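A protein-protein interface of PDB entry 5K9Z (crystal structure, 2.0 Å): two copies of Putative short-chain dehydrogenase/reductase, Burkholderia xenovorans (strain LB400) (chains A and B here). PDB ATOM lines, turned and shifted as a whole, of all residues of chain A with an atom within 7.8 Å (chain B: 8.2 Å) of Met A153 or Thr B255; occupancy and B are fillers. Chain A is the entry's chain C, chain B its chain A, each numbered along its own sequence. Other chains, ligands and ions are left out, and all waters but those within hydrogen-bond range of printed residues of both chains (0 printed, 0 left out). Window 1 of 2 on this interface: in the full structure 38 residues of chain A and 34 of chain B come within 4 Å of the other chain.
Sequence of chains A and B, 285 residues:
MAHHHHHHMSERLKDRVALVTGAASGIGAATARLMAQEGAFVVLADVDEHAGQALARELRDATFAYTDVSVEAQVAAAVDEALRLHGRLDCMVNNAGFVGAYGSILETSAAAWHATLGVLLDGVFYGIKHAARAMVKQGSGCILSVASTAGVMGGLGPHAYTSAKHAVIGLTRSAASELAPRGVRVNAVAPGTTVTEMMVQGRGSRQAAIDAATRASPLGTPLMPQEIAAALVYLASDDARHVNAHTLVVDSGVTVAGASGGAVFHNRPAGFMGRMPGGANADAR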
ATOM      1  N   SER A 148      13.204 -25.459  30.773  1.00  0.00           N
ATOM      2  CA  SER A 148      14.006 -26.675  30.912  1.00  0.00           C
ATOM      3  C   SER A 148      15.467 -26.267  30.994  1.00  0.00           C
ATOM      4  O   SER A 148      15.846 -25.195  30.522  1.00  0.00           O
ATOM      5  CB  SER A 148      13.811 -27.621  29.721  1.00  0.00           C
ATOM      6  OG  SER A 148      14.836 -28.582  29.678  1.00  0.00           O
ATOM      7  N   THR A 149      16.299 -27.169  31.533  1.00  0.00           N
ATOM      8  CA  THR A 149      17.739 -26.970  31.452  1.00  0.00           C
ATOM      9  C   THR A 149      18.203 -26.854  30.006  1.00  0.00           C
ATOM     10  O   THR A 149      19.224 -26.208  29.731  1.00  0.00           O
ATOM     11  CB  THR A 149      18.487 -28.127  32.140  1.00  0.00           C
ATOM     12  OG1 THR A 149      17.988 -29.375  31.659  1.00  0.00           O
ATOM     13  CG2 THR A 149      18.279 -28.083  33.623  1.00  0.00           C
ATOM     14  N   ALA A 150      17.462 -27.451  29.064  1.00  0.00           N
ATOM     15  CA  ALA A 150      17.767 -27.281  27.650  1.00  0.00           C
ATOM     16  C   ALA A 150      17.583 -25.840  27.178  1.00  0.00           C
ATOM     17  O   ALA A 150      18.078 -25.486  26.100  1.00  0.00           O
ATOM     18  CB  ALA A 150      16.895 -28.227  26.814  1.00  0.00           C
ATOM     19  N   GLY A 151      16.933 -24.998  27.972  1.00  0.00           N
ATOM     20  CA  GLY A 151      16.875 -23.576  27.674  1.00  0.00           C
ATOM     21  C   GLY A 151      18.070 -22.793  28.155  1.00  0.00           C
ATOM     22  O   GLY A 151      18.199 -21.609  27.833  1.00  0.00           O
ATOM     23  N   VAL A 152      18.972 -23.452  28.874  1.00  0.00           N
ATOM     24  CA  VAL A 152      20.125 -22.797  29.467  1.00  0.00           C
ATOM     25  C   VAL A 152      21.441 -23.188  28.792  1.00  0.00           C
ATOM     26  O   VAL A 152      22.399 -22.398  28.837  1.00  0.00           O
ATOM     27  CB  VAL A 152      20.164 -23.113  30.984  1.00  0.00           C
ATOM     28  CG1 VAL A 152      21.542 -22.991  31.578  1.00  0.00           C
ATOM     29  CG2 VAL A 152      19.148 -22.228  31.737  1.00  0.00           C
ATOM     30  N   MET A 153      21.501 -24.336  28.115  1.00  0.00           N
ATOM     31  CA  MET A 153      22.699 -24.740  27.390  1.00  0.00           C
ATOM     32  C   MET A 153      22.317 -25.820  26.383  1.00  0.00           C
ATOM     33  O   MET A 153      21.200 -26.351  26.405  1.00  0.00           O
ATOM     34  CB  MET A 153      23.785 -25.204  28.368  1.00  0.00           C
ATOM     35  CG  MET A 153      23.427 -26.460  29.150  1.00  0.00           C
ATOM     36  SD  MET A 153      24.763 -27.127  30.221  1.00  0.00           S
ATOM     37  CE  MET A 153      26.025 -27.454  28.995  1.00  0.00           C
ATOM     38  N   GLY A 154      23.267 -26.129  25.479  1.00  0.00           N
ATOM     39  CA  GLY A 154      23.087 -27.215  24.534  1.00  0.00           C
ATOM     40  C   GLY A 154      23.483 -28.572  25.129  1.00  0.00           C
ATOM     41  O   GLY A 154      24.018 -28.678  26.236  1.00  0.00           O
ATOM     42  N   GLY A 155      23.183 -29.633  24.370  1.00  0.00           N
ATOM     43  CA  GLY A 155      23.503 -30.987  24.760  1.00  0.00           C
ATOM     44  C   GLY A 155      22.543 -31.632  25.747  1.00  0.00           C
ATOM     45  O   GLY A 155      22.771 -32.779  26.142  1.00  0.00           O
ATOM     46  N   LEU A 156      21.457 -30.960  26.124  1.00  0.00           N
ATOM     47  CA  LEU A 156      20.526 -31.477  27.124  1.00  0.00           C
ATOM     48  C   LEU A 156      19.151 -31.820  26.556  1.00  0.00           C
ATOM     49  O   LEU A 156      18.270 -32.251  27.307  1.00  0.00           O
ATOM     50  CB  LEU A 156      20.401 -30.470  28.285  1.00  0.00           C
ATOM     51  CG  LEU A 156      21.678 -30.296  29.125  1.00  0.00           C
ATOM     52  CD1 LEU A 156      21.525 -29.294  30.267  1.00  0.00           C
ATOM     53  CD2 LEU A 156      22.134 -31.652  29.657  1.00  0.00           C
ATOM     54  N   GLY A 157      18.913 -31.559  25.283  1.00  0.00           N
ATOM     55  CA  GLY A 157      17.668 -31.937  24.641  1.00  0.00           C
ATOM     56  C   GLY A 157      17.816 -31.867  23.140  1.00  0.00           C
ATOM     57  O   GLY A 157      18.880 -31.511  22.621  1.00  0.00           O
ATOM     58  N   PRO A 158      16.761 -32.241  22.412  1.00  0.00           N
ATOM     59  CA  PRO A 158      16.780 -32.139  20.949  1.00  0.00           C
ATOM     60  C   PRO A 158      16.957 -30.701  20.477  1.00  0.00           C
ATOM     61  O   PRO A 158      16.810 -29.744  21.238  1.00  0.00           O
ATOM     62  CB  PRO A 158      15.407 -32.687  20.534  1.00  0.00           C
ATOM     63  CG  PRO A 158      14.982 -33.551  21.682  1.00  0.00           C
ATOM     64  CD  PRO A 158      15.541 -32.894  22.911  1.00  0.00           C
ATOM     65  N   THR A 162      15.692 -27.500  22.348  1.00  0.00           N
ATOM     66  CA  THR A 162      16.672 -26.601  22.942  1.00  0.00           C
ATOM     67  C   THR A 162      16.459 -25.164  22.458  1.00  0.00           C
ATOM     68  O   THR A 162      16.511 -24.220  23.254  1.00  0.00           O
ATOM     69  CB  THR A 162      18.083 -27.097  22.616  1.00  0.00           C
ATOM     70  OG1 THR A 162      18.302 -28.412  23.186  1.00  0.00           O
ATOM     71  CG2 THR A 162      19.125 -26.128  23.128  1.00  0.00           C
ATOM     72  N   SER A 163      16.203 -24.978  21.158  1.00  0.00           N
ATOM     73  CA  SER A 163      15.997 -23.632  20.639  1.00  0.00           C
ATOM     74  C   SER A 163      14.743 -23.001  21.240  1.00  0.00           C
ATOM     75  O   SER A 163      14.755 -21.832  21.662  1.00  0.00           O
ATOM     76  CB  SER A 163      15.916 -23.693  19.116  1.00  0.00           C
ATOM     77  OG  SER A 163      15.825 -22.416  18.535  1.00  0.00           O
ATOM     78  N   LYS A 165      13.261 -23.700  24.085  1.00  0.00           N
ATOM     79  CA  LYS A 165      13.388 -23.414  25.512  1.00  0.00           C
ATOM     80  C   LYS A 165      14.274 -22.197  25.754  1.00  0.00           C
ATOM     81  O   LYS A 165      14.016 -21.423  26.683  1.00  0.00           O
ATOM     82  CB  LYS A 165      13.927 -24.654  26.245  1.00  0.00           C
ATOM     83  CG  LYS A 165      12.960 -25.837  26.226  1.00  0.00           C
ATOM     84  CD  LYS A 165      11.686 -25.562  27.043  1.00  0.00           C
ATOM     85  CE  LYS A 165      10.730 -26.765  27.028  1.00  0.00           C
ATOM     86  NZ  LYS A 165       9.493 -26.525  27.825  1.00  0.00           N
ATOM     87  N   HIS A 166      15.334 -22.020  24.939  1.00  0.00           N
ATOM     88  CA  HIS A 166      16.113 -20.785  24.984  1.00  0.00           C
ATOM     89  C   HIS A 166      15.240 -19.583  24.651  1.00  0.00           C
ATOM     90  O   HIS A 166      15.342 -18.535  25.294  1.00  0.00           O
ATOM     91  CB  HIS A 166      17.301 -20.843  24.010  1.00  0.00           C
ATOM     92  CG  HIS A 166      18.535 -21.496  24.565  1.00  0.00           C
ATOM     93  ND1 HIS A 166      18.649 -22.861  24.733  1.00  0.00           N
ATOM     94  CD2 HIS A 166      19.727 -20.972  24.947  1.00  0.00           C
ATOM     95  CE1 HIS A 166      19.847 -23.147  25.216  1.00  0.00           C
ATOM     96  NE2 HIS A 166      20.530 -22.024  25.331  1.00  0.00           N
ATOM     97  N   ILE A 169      13.035 -18.578  27.605  1.00  0.00           N
ATOM     98  CA  ILE A 169      13.752 -17.769  28.583  1.00  0.00           C
ATOM     99  C   ILE A 169      13.940 -16.345  28.067  1.00  0.00           C
ATOM    100  O   ILE A 169      13.768 -15.376  28.815  1.00  0.00           O
ATOM    101  CB  ILE A 169      15.079 -18.452  28.955  1.00  0.00           C
ATOM    102  CG1 ILE A 169      14.773 -19.690  29.806  1.00  0.00           C
ATOM    103  CG2 ILE A 169      16.013 -17.475  29.691  1.00  0.00           C
ATOM    104  CD1 ILE A 169      15.983 -20.516  30.186  1.00  0.00           C
ATOM    105  N   ASP A 251      17.793 -28.838  38.880  1.00  0.00           N
ATOM    106  CA  ASP A 251      18.470 -29.858  38.082  1.00  0.00           C
ATOM    107  C   ASP A 251      19.602 -30.547  38.839  1.00  0.00           C
ATOM    108  O   ASP A 251      20.507 -31.089  38.201  1.00  0.00           O
ATOM    109  CB  ASP A 251      19.020 -29.223  36.780  1.00  0.00           C
ATOM    110  CG  ASP A 251      20.276 -28.355  37.013  1.00  0.00           C
ATOM    111  OD1 ASP A 251      20.549 -27.912  38.153  1.00  0.00           O
ATOM    112  OD2 ASP A 251      20.986 -28.082  36.029  1.00  0.00           O
ATOM    113  N   VAL A 254      23.435 -29.737  37.567  1.00  0.00           N
ATOM    114  CA  VAL A 254      24.148 -30.253  36.399  1.00  0.00           C
ATOM    115  C   VAL A 254      24.623 -29.124  35.480  1.00  0.00           C
ATOM    116  O   VAL A 254      25.733 -29.186  34.931  1.00  0.00           O
ATOM    117  CB  VAL A 254      23.267 -31.272  35.645  1.00  0.00           C
ATOM    118  CG1 VAL A 254      23.830 -31.540  34.263  1.00  0.00           C
ATOM    119  CG2 VAL A 254      23.167 -32.575  36.452  1.00  0.00           C
ATOM    120  N   THR A 255      23.787 -28.097  35.262  1.00  0.00           N
ATOM    121  CA  THR A 255      24.136 -27.084  34.263  1.00  0.00           C
ATOM    122  C   THR A 255      25.305 -26.209  34.720  1.00  0.00           C
ATOM    123  O   THR A 255      26.056 -25.708  33.879  1.00  0.00           O
ATOM    124  CB  THR A 255      22.924 -26.197  33.916  1.00  0.00           C
ATOM    125  OG1 THR A 255      22.419 -25.558  35.096  1.00  0.00           O
ATOM    126  CG2 THR A 255      21.808 -27.009  33.263  1.00  0.00           C
ATOM    127  N   VAL A 256      25.480 -26.020  36.024  1.00  0.00           N
ATOM    128  CA  VAL A 256      26.515 -25.131  36.547  1.00  0.00           C
ATOM    129  C   VAL A 256      27.589 -25.856  37.351  1.00  0.00           C
ATOM    130  O   VAL A 256      28.601 -25.225  37.712  1.00  0.00           O
ATOM    131  CB  VAL A 256      25.913 -23.984  37.393  1.00  0.00           C
ATOM    132  CG1 VAL A 256      25.139 -22.993  36.508  1.00  0.00           C
ATOM    133  CG2 VAL A 256      25.024 -24.534  38.478  1.00  0.00           C
ATOM    134  N   GLY A 258      28.244 -29.517  36.665  1.00  0.00           N
ATOM    135  CA  GLY A 258      28.681 -30.719  35.990  1.00  0.00           C
ATOM    136  C   GLY A 258      27.774 -31.903  36.248  1.00  0.00           C
ATOM    137  O   GLY A 258      27.095 -32.002  37.271  1.00  0.00           O
ATOM    138  N   SER B 148      39.867 -19.211  32.523  1.00  0.00           N
ATOM    139  CA  SER B 148      39.669 -20.638  32.307  1.00  0.00           C
ATOM    140  C   SER B 148      38.173 -20.853  32.212  1.00  0.00           C
ATOM    141  O   SER B 148      37.399 -20.044  32.724  1.00  0.00           O
ATOM    142  CB  SER B 148      40.224 -21.478  33.467  1.00  0.00           C
ATOM    143  OG  SER B 148      39.708 -22.795  33.411  1.00  0.00           O
ATOM    144  N   THR B 149      37.769 -21.964  31.584  1.00  0.00           N
ATOM    145  CA  THR B 149      36.368 -22.362  31.677  1.00  0.00           C
ATOM    146  C   THR B 149      35.946 -22.633  33.118  1.00  0.00           C
ATOM    147  O   THR B 149      34.756 -22.536  33.429  1.00  0.00           O
ATOM    148  CB  THR B 149      36.081 -23.583  30.792  1.00  0.00           C
ATOM    149  OG1 THR B 149      37.066 -24.588  31.014  1.00  0.00           O
ATOM    150  CG2 THR B 149      36.071 -23.187  29.321  1.00  0.00           C
ATOM    151  N   ALA B 150      36.888 -22.961  34.012  1.00  0.00           N
ATOM    152  CA  ALA B 150      36.546 -23.033  35.431  1.00  0.00           C
ATOM    153  C   ALA B 150      36.128 -21.678  36.001  1.00  0.00           C
ATOM    154  O   ALA B 150      35.652 -21.624  37.139  1.00  0.00           O
ATOM    155  CB  ALA B 150      37.714 -23.605  36.252  1.00  0.00           C
ATOM    156  N   GLY B 151      36.311 -20.590  35.264  1.00  0.00           N
ATOM    157  CA  GLY B 151      35.743 -19.333  35.710  1.00  0.00           C
ATOM    158  C   GLY B 151      34.295 -19.124  35.328  1.00  0.00           C
ATOM    159  O   GLY B 151      33.682 -18.166  35.812  1.00  0.00           O
ATOM    160  N   VAL B 152      33.737 -20.001  34.491  1.00  0.00           N
ATOM    161  CA  VAL B 152      32.342 -19.888  34.069  1.00  0.00           C
ATOM    162  C   VAL B 152      31.469 -21.030  34.588  1.00  0.00           C
ATOM    163  O   VAL B 152      30.237 -20.916  34.513  1.00  0.00           O
ATOM    164  CB  VAL B 152      32.184 -19.762  32.534  1.00  0.00           C
ATOM    165  CG1 VAL B 152      32.977 -18.578  31.999  1.00  0.00           C
ATOM    166  CG2 VAL B 152      32.569 -21.028  31.829  1.00  0.00           C
ATOM    167  N   MET B 153      32.049 -22.142  35.060  1.00  0.00           N
ATOM    168  CA  MET B 153      31.209 -23.152  35.699  1.00  0.00           C
ATOM    169  C   MET B 153      32.037 -24.028  36.632  1.00  0.00           C
ATOM    170  O   MET B 153      33.270 -24.068  36.562  1.00  0.00           O
ATOM    171  CB  MET B 153      30.499 -24.045  34.690  1.00  0.00           C
ATOM    172  CG  MET B 153      31.366 -25.013  33.971  1.00  0.00           C
ATOM    173  SD  MET B 153      30.265 -26.067  33.011  1.00  0.00           S
ATOM    174  CE  MET B 153      29.202 -26.734  34.285  1.00  0.00           C
ATOM    175  N   GLY B 154      31.320 -24.746  37.502  1.00  0.00           N
ATOM    176  CA  GLY B 154      31.947 -25.646  38.442  1.00  0.00           C
ATOM    177  C   GLY B 154      32.170 -27.020  37.853  1.00  0.00           C
ATOM    178  O   GLY B 154      31.688 -27.347  36.765  1.00  0.00           O
ATOM    179  N   LEU B 156      35.000 -28.271  36.852  1.00  0.00           N
ATOM    180  CA  LEU B 156      36.044 -28.334  35.835  1.00  0.00           C
ATOM    181  C   LEU B 156      37.446 -28.131  36.368  1.00  0.00           C
ATOM    182  O   LEU B 156      38.403 -28.373  35.627  1.00  0.00           O
ATOM    183  CB  LEU B 156      35.805 -27.269  34.761  1.00  0.00           C
ATOM    184  CG  LEU B 156      34.587 -27.439  33.867  1.00  0.00           C
ATOM    185  CD1 LEU B 156      34.515 -26.245  32.943  1.00  0.00           C
ATOM    186  CD2 LEU B 156      34.682 -28.755  33.074  1.00  0.00           C
ATOM    187  N   ALA B 190      39.062 -17.666  28.100  1.00  0.00           N
ATOM    188  CA  ALA B 190      38.751 -18.810  28.954  1.00  0.00           C
ATOM    189  C   ALA B 190      39.118 -20.084  28.199  1.00  0.00           C
ATOM    190  O   ALA B 190      38.262 -20.693  27.527  1.00  0.00           O
ATOM    191  CB  ALA B 190      37.282 -18.809  29.369  1.00  0.00           C
ATOM    192  N   PRO B 191      40.380 -20.517  28.282  1.00  0.00           N
ATOM    193  CA  PRO B 191      40.760 -21.815  27.705  1.00  0.00           C
ATOM    194  C   PRO B 191      40.056 -22.950  28.420  1.00  0.00           C
ATOM    195  O   PRO B 191      39.808 -22.901  29.628  1.00  0.00           O
ATOM    196  CB  PRO B 191      42.280 -21.886  27.929  1.00  0.00           C
ATOM    197  CG  PRO B 191      42.699 -20.503  28.348  1.00  0.00           C
ATOM    198  CD  PRO B 191      41.506 -19.832  28.936  1.00  0.00           C
ATOM    199  N   GLY B 192      39.769 -24.004  27.661  1.00  0.00           N
ATOM    200  CA  GLY B 192      39.317 -25.230  28.267  1.00  0.00           C
ATOM    201  C   GLY B 192      40.396 -25.863  29.119  1.00  0.00           C
ATOM    202  O   GLY B 192      41.593 -25.618  28.954  1.00  0.00           O
ATOM    203  N   THR B 193      39.955 -26.680  30.073  1.00  0.00           N
ATOM    204  CA  THR B 193      40.878 -27.422  30.923  1.00  0.00           C
ATOM    205  C   THR B 193      41.434 -28.609  30.132  1.00  0.00           C
ATOM    206  O   THR B 193      41.229 -29.779  30.451  1.00  0.00           O
ATOM    207  CB  THR B 193      40.189 -27.845  32.214  1.00  0.00           C
ATOM    208  OG1 THR B 193      39.102 -28.732  31.923  1.00  0.00           O
ATOM    209  CG2 THR B 193      39.648 -26.606  32.938  1.00  0.00           C
ATOM    210  N   PRO B 218      35.347 -32.191  21.765  1.00  0.00           N
ATOM    211  CA  PRO B 218      34.320 -32.695  20.835  1.00  0.00           C
ATOM    212  C   PRO B 218      34.749 -32.641  19.381  1.00  0.00           C
ATOM    213  O   PRO B 218      34.253 -33.431  18.567  1.00  0.00           O
ATOM    214  CB  PRO B 218      33.124 -31.769  21.102  1.00  0.00           C
ATOM    215  CG  PRO B 218      33.289 -31.338  22.509  1.00  0.00           C
ATOM    216  CD  PRO B 218      34.787 -31.219  22.722  1.00  0.00           C
ATOM    217  N   VAL B 249      35.639 -17.727  25.058  1.00  0.00           N
ATOM    218  CA  VAL B 249      35.776 -19.114  25.496  1.00  0.00           C
ATOM    219  C   VAL B 249      36.398 -19.938  24.375  1.00  0.00           C
ATOM    220  O   VAL B 249      35.912 -19.928  23.240  1.00  0.00           O
ATOM    221  CB  VAL B 249      34.408 -19.696  25.911  1.00  0.00           C
ATOM    222  CG1 VAL B 249      34.525 -21.190  26.262  1.00  0.00           C
ATOM    223  CG2 VAL B 249      33.798 -18.902  27.074  1.00  0.00           C
ATOM    224  N   VAL B 250      37.461 -20.675  24.693  1.00  0.00           N
ATOM    225  CA  VAL B 250      38.115 -21.529  23.701  1.00  0.00           C
ATOM    226  C   VAL B 250      38.158 -22.945  24.259  1.00  0.00           C
ATOM    227  O   VAL B 250      39.160 -23.364  24.861  1.00  0.00           O
ATOM    228  CB  VAL B 250      39.537 -21.030  23.351  1.00  0.00           C
ATOM    229  CG1 VAL B 250      40.128 -21.850  22.198  1.00  0.00           C
ATOM    230  CG2 VAL B 250      39.526 -19.530  23.011  1.00  0.00           C
ATOM    231  N   ASP B 251      37.068 -23.699  24.080  1.00  0.00           N
ATOM    232  CA  ASP B 251      37.007 -25.001  24.737  1.00  0.00           C
ATOM    233  C   ASP B 251      36.290 -26.062  23.906  1.00  0.00           C
ATOM    234  O   ASP B 251      35.814 -27.053  24.472  1.00  0.00           O
ATOM    235  CB  ASP B 251      36.318 -24.901  26.112  1.00  0.00           C
ATOM    236  CG  ASP B 251      34.796 -24.725  26.003  1.00  0.00           C
ATOM    237  OD1 ASP B 251      34.303 -24.243  24.950  1.00  0.00           O
ATOM    238  OD2 ASP B 251      34.088 -25.116  26.961  1.00  0.00           O
ATOM    239  N   SER B 252      36.175 -25.867  22.592  1.00  0.00           N
ATOM    240  CA  SER B 252      35.490 -26.786  21.682  1.00  0.00           C
ATOM    241  C   SER B 252      34.013 -26.952  22.024  1.00  0.00           C
ATOM    242  O   SER B 252      33.384 -27.896  21.560  1.00  0.00           O
ATOM    243  CB  SER B 252      36.167 -28.166  21.652  1.00  0.00           C
ATOM    244  OG  SER B 252      37.517 -28.066  21.225  1.00  0.00           O
ATOM    245  N   GLY B 253      33.448 -26.042  22.820  1.00  0.00           N
ATOM    246  CA  GLY B 253      32.031 -26.077  23.127  1.00  0.00           C
ATOM    247  C   GLY B 253      31.625 -26.899  24.331  1.00  0.00           C
ATOM    248  O   GLY B 253      30.429 -27.166  24.497  1.00  0.00           O
ATOM    249  N   VAL B 254      32.577 -27.343  25.160  1.00  0.00           N
ATOM    250  CA  VAL B 254      32.247 -28.281  26.234  1.00  0.00           C
ATOM    251  C   VAL B 254      31.311 -27.646  27.262  1.00  0.00           C
ATOM    252  O   VAL B 254      30.351 -28.279  27.718  1.00  0.00           O
ATOM    253  CB  VAL B 254      33.533 -28.811  26.898  1.00  0.00           C
ATOM    254  CG1 VAL B 254      33.206 -29.472  28.222  1.00  0.00           C
ATOM    255  CG2 VAL B 254      34.222 -29.814  25.989  1.00  0.00           C
ATOM    256  N   THR B 255      31.568 -26.396  27.651  1.00  0.00           N
ATOM    257  CA  THR B 255      30.801 -25.835  28.762  1.00  0.00           C
ATOM    258  C   THR B 255      29.355 -25.533  28.381  1.00  0.00           C
ATOM    259  O   THR B 255      28.478 -25.595  29.247  1.00  0.00           O
ATOM    260  CB  THR B 255      31.464 -24.570  29.314  1.00  0.00           C
ATOM    261  OG1 THR B 255      31.591 -23.572  28.285  1.00  0.00           O
ATOM    262  CG2 THR B 255      32.829 -24.907  29.890  1.00  0.00           C
ATOM    263  N   VAL B 256      29.076 -25.208  27.117  1.00  0.00           N
ATOM    264  CA  VAL B 256      27.719 -24.842  26.709  1.00  0.00           C
ATOM    265  C   VAL B 256      27.090 -25.834  25.745  1.00  0.00           C
ATOM    266  O   VAL B 256      25.909 -25.660  25.405  1.00  0.00           O
ATOM    267  CB  VAL B 256      27.661 -23.430  26.081  1.00  0.00           C
ATOM    268  CG1 VAL B 256      27.944 -22.345  27.114  1.00  0.00           C
ATOM    269  CG2 VAL B 256      28.602 -23.319  24.894  1.00  0.00           C
ATOM    270  N   ALA B 257      27.837 -26.831  25.254  1.00  0.00           N
ATOM    271  CA  ALA B 257      27.340 -27.704  24.195  1.00  0.00           C
ATOM    272  C   ALA B 257      27.927 -29.117  24.274  1.00  0.00           C
ATOM    273  O   ALA B 257      28.307 -29.684  23.245  1.00  0.00           O
ATOM    274  CB  ALA B 257      27.633 -27.116  22.817  1.00  0.00           C
ATOM    275  N   GLY B 258      28.108 -29.661  25.478  1.00  0.00           N
ATOM    276  CA  GLY B 258      28.555 -31.050  25.619  1.00  0.00           C
ATOM    277  C   GLY B 258      28.169 -32.043  24.520  1.00  0.00           C
ATOM    278  O   GLY B 258      26.999 -32.435  24.388  1.00  0.00           O
ATOM    279  N   ALA B 259      29.150 -32.467  23.715  1.00  0.00           N
ATOM    280  CA  ALA B 259      28.840 -33.290  22.546  1.00  0.00           C
ATOM    281  C   ALA B 259      28.525 -34.739  22.909  1.00  0.00           C
ATOM    282  O   ALA B 259      27.737 -35.393  22.206  1.00  0.00           O
ATOM    283  CB  ALA B 259      29.992 -33.240  21.541  1.00  0.00           C
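N of Gly B154 lies within hydrogen-bond range of O of Val A256, 2.8 Å away. The backbone NH of Gly A154 sits at hydrogen-bond distance from the backbone carbonyl oxygen of Val B256, at 2.7 Å.
The backbone NH (N) of Thr B255 is in hydrogen-bond range of the side-chain carboxylate (OD2) of Asp B251 (2.9 Å). OD2 of Asp A251 lies within hydrogen-bond range of N of Thr A255, 2.9 Å away.
Met A153 touches Thr B255 (CE to O, 3.1 Å). Met A153 touches Val B256 (CB to O, 3.7 Å). Gly B258 touches Gly A155. O of Thr A255 touches CE of Met B153, at 3.3 Å. Val A256 touches Met B153 (C to CE, 3.6 Å). CE of Met B153 touches N of Gly A258 (3.8 Å).
Gly A151 touches none of the printed residues of chain B. Of chain B, only Thr B255 (3.1 Å) and Val B256 (3.7 Å) come within 4 Å of Met A153. Of the printed residues of chain B, Thr A255 touches Met B153 (3.3 Å). Of the printed residues of chain A, Gly B154 touches Val A256 (2.8 Å). Leu B156 touches none of the printed residues of chain A. Of chain A, only Met A153 (3.1 Å) comes within 4 Å of Thr B255. Printed residues of chain A within 4 Å of Val B256: Met A153 and Gly A154. The nearest residue of chain B that does not touch Met A153 is Ala B257 (4.2 Å). The nearest printed residue of chain A that does not touch Gly B258 is Gly A154 (4.3 Å).
Printed residues of chain B that touch a printed residue of chain A: Met B153, Gly B154, Thr B255, Val B256 and Gly B258. Hydrophobic or aromatic side chains of chain B that line the printed part of chain A: Met B153.
Met A153 touches Thr B255, and with the chains exchanged Thr A255 touches Met B153. Met A153 touches Val B256, and with the chains exchanged Val A256 touches Met B153. Gly A154 touches Val B256, and with the chains exchanged Val A256 touches Gly B154. Gly A258 touches Met B153, but with the chains exchanged Met A153 does not touch Gly B258 (4.6 Å). Of the 8 pairs that touch across the chains among the printed residues, 6 have their exchanged pair printed and touching as well.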
